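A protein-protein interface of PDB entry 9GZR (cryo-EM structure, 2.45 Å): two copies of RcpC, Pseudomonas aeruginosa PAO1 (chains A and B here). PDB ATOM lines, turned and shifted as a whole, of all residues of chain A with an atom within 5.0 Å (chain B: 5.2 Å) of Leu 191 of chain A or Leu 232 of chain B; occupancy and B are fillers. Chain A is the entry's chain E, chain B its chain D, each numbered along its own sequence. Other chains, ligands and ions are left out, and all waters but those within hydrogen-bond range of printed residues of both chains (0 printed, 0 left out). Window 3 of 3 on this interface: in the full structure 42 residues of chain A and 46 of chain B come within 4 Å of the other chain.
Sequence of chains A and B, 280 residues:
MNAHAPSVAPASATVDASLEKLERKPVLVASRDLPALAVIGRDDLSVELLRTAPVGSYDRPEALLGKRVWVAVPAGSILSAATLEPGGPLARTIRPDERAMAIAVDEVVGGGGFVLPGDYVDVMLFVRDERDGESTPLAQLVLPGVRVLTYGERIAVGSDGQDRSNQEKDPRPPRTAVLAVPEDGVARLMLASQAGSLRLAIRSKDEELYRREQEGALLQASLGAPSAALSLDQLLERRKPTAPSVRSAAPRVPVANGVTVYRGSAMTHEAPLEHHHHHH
No position is printed for both chains.
Of the 12 pairs that touch across the chains among the printed residues, none has its exchanged pair printed and touching as well.
The side-chain carboxylate (OD1) of Asp 233 of chain B lies within salt-bridge range of the guanidinium group (NE) of Arg 131 of chain A (2.6 Å).
Of the printed residues of chain B, Val 127 of chain A touches Leu 232 and Leu 236.
Of the printed residues of chain B, Arg 188 of chain A touches Leu 230 (3.8 Å) and Leu 235 (3.4 Å).
Leu 191 of chain A touches five residues of chain B.
Of chain A, only Val 127 and Leu 191 come within 4 Å of Leu 232 of chain B.
The nearest residue of chain B that does not touch Leu 191 of chain A is Leu 138 of chain B (4.1 Å).
The nearest residue of chain A that does not touch Leu 232 of chain B is Ala 195 of chain A (4.3 Å).
The nearest printed residue of chain A that does not touch Ser 231 of chain B is Arg 131 of chain A (6.8 Å).
Among the printed residues, merely in contact across the chains: Val 127 of chain A with Leu 232 of chain B (3.9 Å), Val 127 of chain A with Leu 236 of chain B (3.7 Å), Ala 187 of chain A with Ala 139 of chain B (3.97 Å), Arg 188 of chain A with Leu 230 of chain B (3.8 Å), Arg 188 of chain A with Leu 235 of chain B (3.4 Å), Leu 191 of chain A with Phe 126 of chain B (3.5 Å), Leu 191 of chain A with Pro 137 of chain B (3.96 Å), Leu 191 of chain A with Leu 230 of chain B (3.7 Å), Leu 191 of chain A with Ser 231 of chain B (3.6 Å), Leu 191 of chain A with Leu 232 of chain B (3.8 Å) and Gln 194 of chain A with Phe 126 of chain B (3.5 Å).
Hydrophobic or aromatic side chains of chain B within 4 Å of the printed part of chain A: Phe 126, Pro 137, Ala 139, Leu 230, Leu 232, Leu 235 and Leu 236.
Among the printed residues, 12 pairs touch across the chains.
The backbone carbonyl oxygen (O) of Ala 139 of chain B lies within hydrogen-bond range of the backbone NH (N) of Leu 230 of chain B (3.2 Å).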
ATOM      1  N   VAL A 127      19.098 -21.776  11.210  1.00  0.00           N
ATOM      2  CA  VAL A 127      17.920 -21.793  10.354  1.00  0.00           C
ATOM      3  C   VAL A 127      17.521 -23.238  10.089  1.00  0.00           C
ATOM      4  O   VAL A 127      18.372 -24.123   9.959  1.00  0.00           O
ATOM      5  CB  VAL A 127      18.175 -21.036   9.027  1.00  0.00           C
ATOM      6  CG1 VAL A 127      19.447 -21.533   8.365  1.00  0.00           C
ATOM      7  CG2 VAL A 127      16.987 -21.148   8.085  1.00  0.00           C
ATOM      8  N   ARG A 131      13.531 -27.307   2.240  1.00  0.00           N
ATOM      9  CA  ARG A 131      13.589 -27.375   0.784  1.00  0.00           C
ATOM     10  C   ARG A 131      12.703 -28.468   0.197  1.00  0.00           C
ATOM     11  O   ARG A 131      11.737 -28.174  -0.514  1.00  0.00           O
ATOM     12  CB  ARG A 131      15.031 -27.600   0.328  1.00  0.00           C
ATOM     13  CG  ARG A 131      15.478 -26.703  -0.810  1.00  0.00           C
ATOM     14  CD  ARG A 131      15.724 -25.288  -0.319  1.00  0.00           C
ATOM     15  NE  ARG A 131      17.012 -24.777  -0.774  1.00  0.00           N
ATOM     16  CZ  ARG A 131      18.170 -25.033  -0.181  1.00  0.00           C
ATOM     17  NH1 ARG A 131      18.241 -25.796   0.897  1.00  0.00           N
ATOM     18  NH2 ARG A 131      19.286 -24.513  -0.684  1.00  0.00           N
ATOM     19  N   ALA A 187      22.583  -7.118   2.164  1.00  0.00           N
ATOM     20  CA  ALA A 187      21.460  -7.996   1.863  1.00  0.00           C
ATOM     21  C   ALA A 187      21.584  -9.325   2.587  1.00  0.00           C
ATOM     22  O   ALA A 187      20.617  -9.767   3.222  1.00  0.00           O
ATOM     23  CB  ALA A 187      21.358  -8.225   0.356  1.00  0.00           C
ATOM     24  N   ARG A 188      22.772  -9.936   2.539  1.00  0.00           N
ATOM     25  CA  ARG A 188      23.027 -11.152   3.300  1.00  0.00           C
ATOM     26  C   ARG A 188      22.504 -11.021   4.722  1.00  0.00           C
ATOM     27  O   ARG A 188      21.607 -11.769   5.137  1.00  0.00           O
ATOM     28  CB  ARG A 188      24.525 -11.454   3.309  1.00  0.00           C
ATOM     29  CG  ARG A 188      24.951 -12.562   2.375  1.00  0.00           C
ATOM     30  CD  ARG A 188      26.459 -12.688   2.337  1.00  0.00           C
ATOM     31  NE  ARG A 188      26.933 -13.831   3.106  1.00  0.00           N
ATOM     32  CZ  ARG A 188      27.119 -15.044   2.605  1.00  0.00           C
ATOM     33  NH1 ARG A 188      26.876 -15.310   1.332  1.00  0.00           N
ATOM     34  NH2 ARG A 188      27.560 -16.013   3.400  1.00  0.00           N
ATOM     35  N   LEU A 189      23.004 -10.024   5.459  1.00  0.00           N
ATOM     36  CA  LEU A 189      22.600  -9.864   6.848  1.00  0.00           C
ATOM     37  C   LEU A 189      21.089  -9.784   6.976  1.00  0.00           C
ATOM     38  O   LEU A 189      20.507 -10.467   7.829  1.00  0.00           O
ATOM     39  CB  LEU A 189      23.254  -8.623   7.451  1.00  0.00           C
ATOM     40  CG  LEU A 189      23.329  -8.578   8.978  1.00  0.00           C
ATOM     41  CD1 LEU A 189      24.041  -9.805   9.512  1.00  0.00           C
ATOM     42  CD2 LEU A 189      24.019  -7.313   9.449  1.00  0.00           C
ATOM     43  N   MET A 190      20.437  -9.017   6.096  1.00  0.00           N
ATOM     44  CA  MET A 190      18.988  -8.888   6.163  1.00  0.00           C
ATOM     45  C   MET A 190      18.326 -10.254   6.144  1.00  0.00           C
ATOM     46  O   MET A 190      17.530 -10.581   7.034  1.00  0.00           O
ATOM     47  CB  MET A 190      18.486  -8.021   5.008  1.00  0.00           C
ATOM     48  CG  MET A 190      17.002  -7.724   5.059  1.00  0.00           C
ATOM     49  SD  MET A 190      16.639  -6.072   5.670  1.00  0.00           S
ATOM     50  CE  MET A 190      14.972  -6.304   6.273  1.00  0.00           C
ATOM     51  N   LEU A 191      18.700 -11.095   5.178  1.00  0.00           N
ATOM     52  CA  LEU A 191      18.132 -12.434   5.111  1.00  0.00           C
ATOM     53  C   LEU A 191      18.369 -13.178   6.416  1.00  0.00           C
ATOM     54  O   LEU A 191      17.429 -13.709   7.025  1.00  0.00           O
ATOM     55  CB  LEU A 191      18.735 -13.194   3.931  1.00  0.00           C
ATOM     56  CG  LEU A 191      17.999 -14.431   3.421  1.00  0.00           C
ATOM     57  CD1 LEU A 191      16.515 -14.177   3.332  1.00  0.00           C
ATOM     58  CD2 LEU A 191      18.550 -14.843   2.072  1.00  0.00           C
ATOM     59  N   ALA A 192      19.610 -13.156   6.904  1.00  0.00           N
ATOM     60  CA  ALA A 192      19.942 -13.904   8.108  1.00  0.00           C
ATOM     61  C   ALA A 192      19.171 -13.375   9.309  1.00  0.00           C
ATOM     62  O   ALA A 192      18.918 -14.106  10.271  1.00  0.00           O
ATOM     63  CB  ALA A 192      21.448 -13.846   8.363  1.00  0.00           C
ATOM     64  N   SER A 193      18.784 -12.100   9.268  1.00  0.00           N
ATOM     65  CA  SER A 193      18.097 -11.524  10.416  1.00  0.00           C
ATOM     66  C   SER A 193      16.643 -11.969  10.468  1.00  0.00           C
ATOM     67  O   SER A 193      16.011 -11.918  11.529  1.00  0.00           O
ATOM     68  CB  SER A 193      18.195 -10.002  10.379  1.00  0.00           C
ATOM     69  OG  SER A 193      17.979  -9.452  11.665  1.00  0.00           O
ATOM     70  N   GLN A 194      16.092 -12.411   9.337  1.00  0.00           N
ATOM     71  CA  GLN A 194      14.668 -12.711   9.292  1.00  0.00           C
ATOM     72  C   GLN A 194      14.362 -14.179   9.032  1.00  0.00           C
ATOM     73  O   GLN A 194      13.268 -14.635   9.379  1.00  0.00           O
ATOM     74  CB  GLN A 194      13.985 -11.853   8.226  1.00  0.00           C
ATOM     75  CG  GLN A 194      14.286 -10.369   8.341  1.00  0.00           C
ATOM     76  CD  GLN A 194      13.382  -9.666   9.328  1.00  0.00           C
ATOM     77  OE1 GLN A 194      13.844  -9.094  10.314  1.00  0.00           O
ATOM     78  NE2 GLN A 194      12.081  -9.705   9.070  1.00  0.00           N
ATOM     79  N   ALA A 195      15.288 -14.923   8.433  1.00  0.00           N
ATOM     80  CA  ALA A 195      15.043 -16.332   8.155  1.00  0.00           C
ATOM     81  C   ALA A 195      15.386 -17.234   9.331  1.00  0.00           C
ATOM     82  O   ALA A 195      15.049 -18.422   9.298  1.00  0.00           O
ATOM     83  CB  ALA A 195      15.837 -16.769   6.925  1.00  0.00           C
ATOM     84  N   GLY A 196      16.035 -16.708  10.358  1.00  0.00           N
ATOM     85  CA  GLY A 196      16.437 -17.537  11.471  1.00  0.00           C
ATOM     86  C   GLY A 196      16.930 -16.712  12.634  1.00  0.00           C
ATOM     87  O   GLY A 196      16.633 -15.522  12.743  1.00  0.00           O
ATOM     88  N   PHE B 126      12.622  -7.408   2.879  1.00  0.00           N
ATOM     89  CA  PHE B 126      12.514  -8.850   3.082  1.00  0.00           C
ATOM     90  C   PHE B 126      11.080  -9.263   2.780  1.00  0.00           C
ATOM     91  O   PHE B 126      10.138  -8.743   3.388  1.00  0.00           O
ATOM     92  CB  PHE B 126      12.904  -9.248   4.505  1.00  0.00           C
ATOM     93  CG  PHE B 126      12.738 -10.714   4.787  1.00  0.00           C
ATOM     94  CD1 PHE B 126      13.630 -11.637   4.277  1.00  0.00           C
ATOM     95  CD2 PHE B 126      11.679 -11.170   5.551  1.00  0.00           C
ATOM     96  CE1 PHE B 126      13.473 -12.984   4.529  1.00  0.00           C
ATOM     97  CE2 PHE B 126      11.520 -12.515   5.802  1.00  0.00           C
ATOM     98  CZ  PHE B 126      12.418 -13.421   5.290  1.00  0.00           C
ATOM     99  N   PRO B 137      12.041 -17.207   1.047  1.00  0.00           N
ATOM    100  CA  PRO B 137      12.498 -15.906   1.558  1.00  0.00           C
ATOM    101  C   PRO B 137      13.458 -15.239   0.583  1.00  0.00           C
ATOM    102  O   PRO B 137      14.193 -15.912  -0.142  1.00  0.00           O
ATOM    103  CB  PRO B 137      13.189 -16.270   2.878  1.00  0.00           C
ATOM    104  CG  PRO B 137      12.648 -17.619   3.229  1.00  0.00           C
ATOM    105  CD  PRO B 137      12.468 -18.307   1.919  1.00  0.00           C
ATOM    106  N   LEU B 138      13.446 -13.907   0.571  1.00  0.00           N
ATOM    107  CA  LEU B 138      14.242 -13.131  -0.368  1.00  0.00           C
ATOM    108  C   LEU B 138      14.616 -11.797   0.261  1.00  0.00           C
ATOM    109  O   LEU B 138      13.975 -11.339   1.207  1.00  0.00           O
ATOM    110  CB  LEU B 138      13.482 -12.889  -1.676  1.00  0.00           C
ATOM    111  CG  LEU B 138      13.541 -13.992  -2.731  1.00  0.00           C
ATOM    112  CD1 LEU B 138      12.262 -14.019  -3.541  1.00  0.00           C
ATOM    113  CD2 LEU B 138      14.749 -13.837  -3.627  1.00  0.00           C
ATOM    114  N   ALA B 139      15.664 -11.176  -0.280  1.00  0.00           N
ATOM    115  CA  ALA B 139      16.103  -9.858   0.153  1.00  0.00           C
ATOM    116  C   ALA B 139      16.625  -9.087  -1.049  1.00  0.00           C
ATOM    117  O   ALA B 139      17.301  -9.654  -1.909  1.00  0.00           O
ATOM    118  CB  ALA B 139      17.184  -9.950   1.232  1.00  0.00           C
ATOM    119  N   LEU B 230      18.555 -12.059  -3.513  1.00  0.00           N
ATOM    120  CA  LEU B 230      19.344 -13.083  -2.843  1.00  0.00           C
ATOM    121  C   LEU B 230      18.424 -14.030  -2.090  1.00  0.00           C
ATOM    122  O   LEU B 230      17.583 -13.588  -1.302  1.00  0.00           O
ATOM    123  CB  LEU B 230      20.350 -12.450  -1.880  1.00  0.00           C
ATOM    124  CG  LEU B 230      21.378 -13.389  -1.252  1.00  0.00           C
ATOM    125  CD1 LEU B 230      22.397 -13.838  -2.282  1.00  0.00           C
ATOM    126  CD2 LEU B 230      22.062 -12.718  -0.077  1.00  0.00           C
ATOM    127  N   SER B 231      18.587 -15.324  -2.330  1.00  0.00           N
ATOM    128  CA  SER B 231      17.769 -16.351  -1.704  1.00  0.00           C
ATOM    129  C   SER B 231      18.585 -17.148  -0.693  1.00  0.00           C
ATOM    130  O   SER B 231      19.810 -17.034  -0.608  1.00  0.00           O
ATOM    131  CB  SER B 231      17.178 -17.281  -2.764  1.00  0.00           C
ATOM    132  OG  SER B 231      16.288 -18.212  -2.178  1.00  0.00           O
ATOM    133  N   LEU B 232      17.877 -17.967   0.090  1.00  0.00           N
ATOM    134  CA  LEU B 232      18.536 -18.830   1.063  1.00  0.00           C
ATOM    135  C   LEU B 232      19.391 -19.898   0.399  1.00  0.00           C
ATOM    136  O   LEU B 232      20.369 -20.353   0.999  1.00  0.00           O
ATOM    137  CB  LEU B 232      17.500 -19.489   1.972  1.00  0.00           C
ATOM    138  CG  LEU B 232      17.388 -18.988   3.412  1.00  0.00           C
ATOM    139  CD1 LEU B 232      16.790 -20.062   4.299  1.00  0.00           C
ATOM    140  CD2 LEU B 232      18.736 -18.541   3.945  1.00  0.00           C
ATOM    141  N   ASP B 233      19.048 -20.307  -0.823  1.00  0.00           N
ATOM    142  CA  ASP B 233      19.832 -21.310  -1.527  1.00  0.00           C
ATOM    143  C   ASP B 233      21.202 -20.791  -1.934  1.00  0.00           C
ATOM    144  O   ASP B 233      22.075 -21.591  -2.285  1.00  0.00           O
ATOM    145  CB  ASP B 233      19.076 -21.795  -2.761  1.00  0.00           C
ATOM    146  CG  ASP B 233      17.666 -22.240  -2.440  1.00  0.00           C
ATOM    147  OD1 ASP B 233      17.293 -22.218  -1.248  1.00  0.00           O
ATOM    148  OD2 ASP B 233      16.929 -22.614  -3.378  1.00  0.00           O
ATOM    149  N   GLN B 234      21.409 -19.478  -1.898  1.00  0.00           N
ATOM    150  CA  GLN B 234      22.703 -18.898  -2.220  1.00  0.00           C
ATOM    151  C   GLN B 234      23.457 -18.451  -0.973  1.00  0.00           C
ATOM    152  O   GLN B 234      24.691 -18.411  -0.977  1.00  0.00           O
ATOM    153  CB  GLN B 234      22.517 -17.728  -3.188  1.00  0.00           C
ATOM    154  CG  GLN B 234      21.763 -18.112  -4.450  1.00  0.00           C
ATOM    155  CD  GLN B 234      21.135 -16.926  -5.146  1.00  0.00           C
ATOM    156  OE1 GLN B 234      21.436 -15.777  -4.831  1.00  0.00           O
ATOM    157  NE2 GLN B 234      20.252 -17.199  -6.097  1.00  0.00           N
ATOM    158  N   LEU B 235      22.737 -18.108   0.096  1.00  0.00           N
ATOM    159  CA  LEU B 235      23.386 -17.830   1.373  1.00  0.00           C
ATOM    160  C   LEU B 235      23.836 -19.119   2.049  1.00  0.00           C
ATOM    161  O   LEU B 235      24.945 -19.201   2.589  1.00  0.00           O
ATOM    162  CB  LEU B 235      22.436 -17.045   2.278  1.00  0.00           C
ATOM    163  CG  LEU B 235      22.870 -16.826   3.727  1.00  0.00           C
ATOM    164  CD1 LEU B 235      23.983 -15.807   3.805  1.00  0.00           C
ATOM    165  CD2 LEU B 235      21.694 -16.388   4.572  1.00  0.00           C
ATOM    166  N   LEU B 236      22.983 -20.145   2.027  1.00  0.00           N
ATOM    167  CA  LEU B 236      23.260 -21.415   2.700  1.00  0.00           C
ATOM    168  C   LEU B 236      24.040 -22.331   1.758  1.00  0.00           C
ATOM    169  O   LEU B 236      23.532 -23.330   1.245  1.00  0.00           O
ATOM    170  CB  LEU B 236      21.966 -22.069   3.160  1.00  0.00           C
ATOM    171  CG  LEU B 236      21.684 -22.117   4.657  1.00  0.00           C
ATOM    172  CD1 LEU B 236      21.819 -20.738   5.272  1.00  0.00           C
ATOM    173  CD2 LEU B 236      20.295 -22.675   4.897  1.00  0.00           C
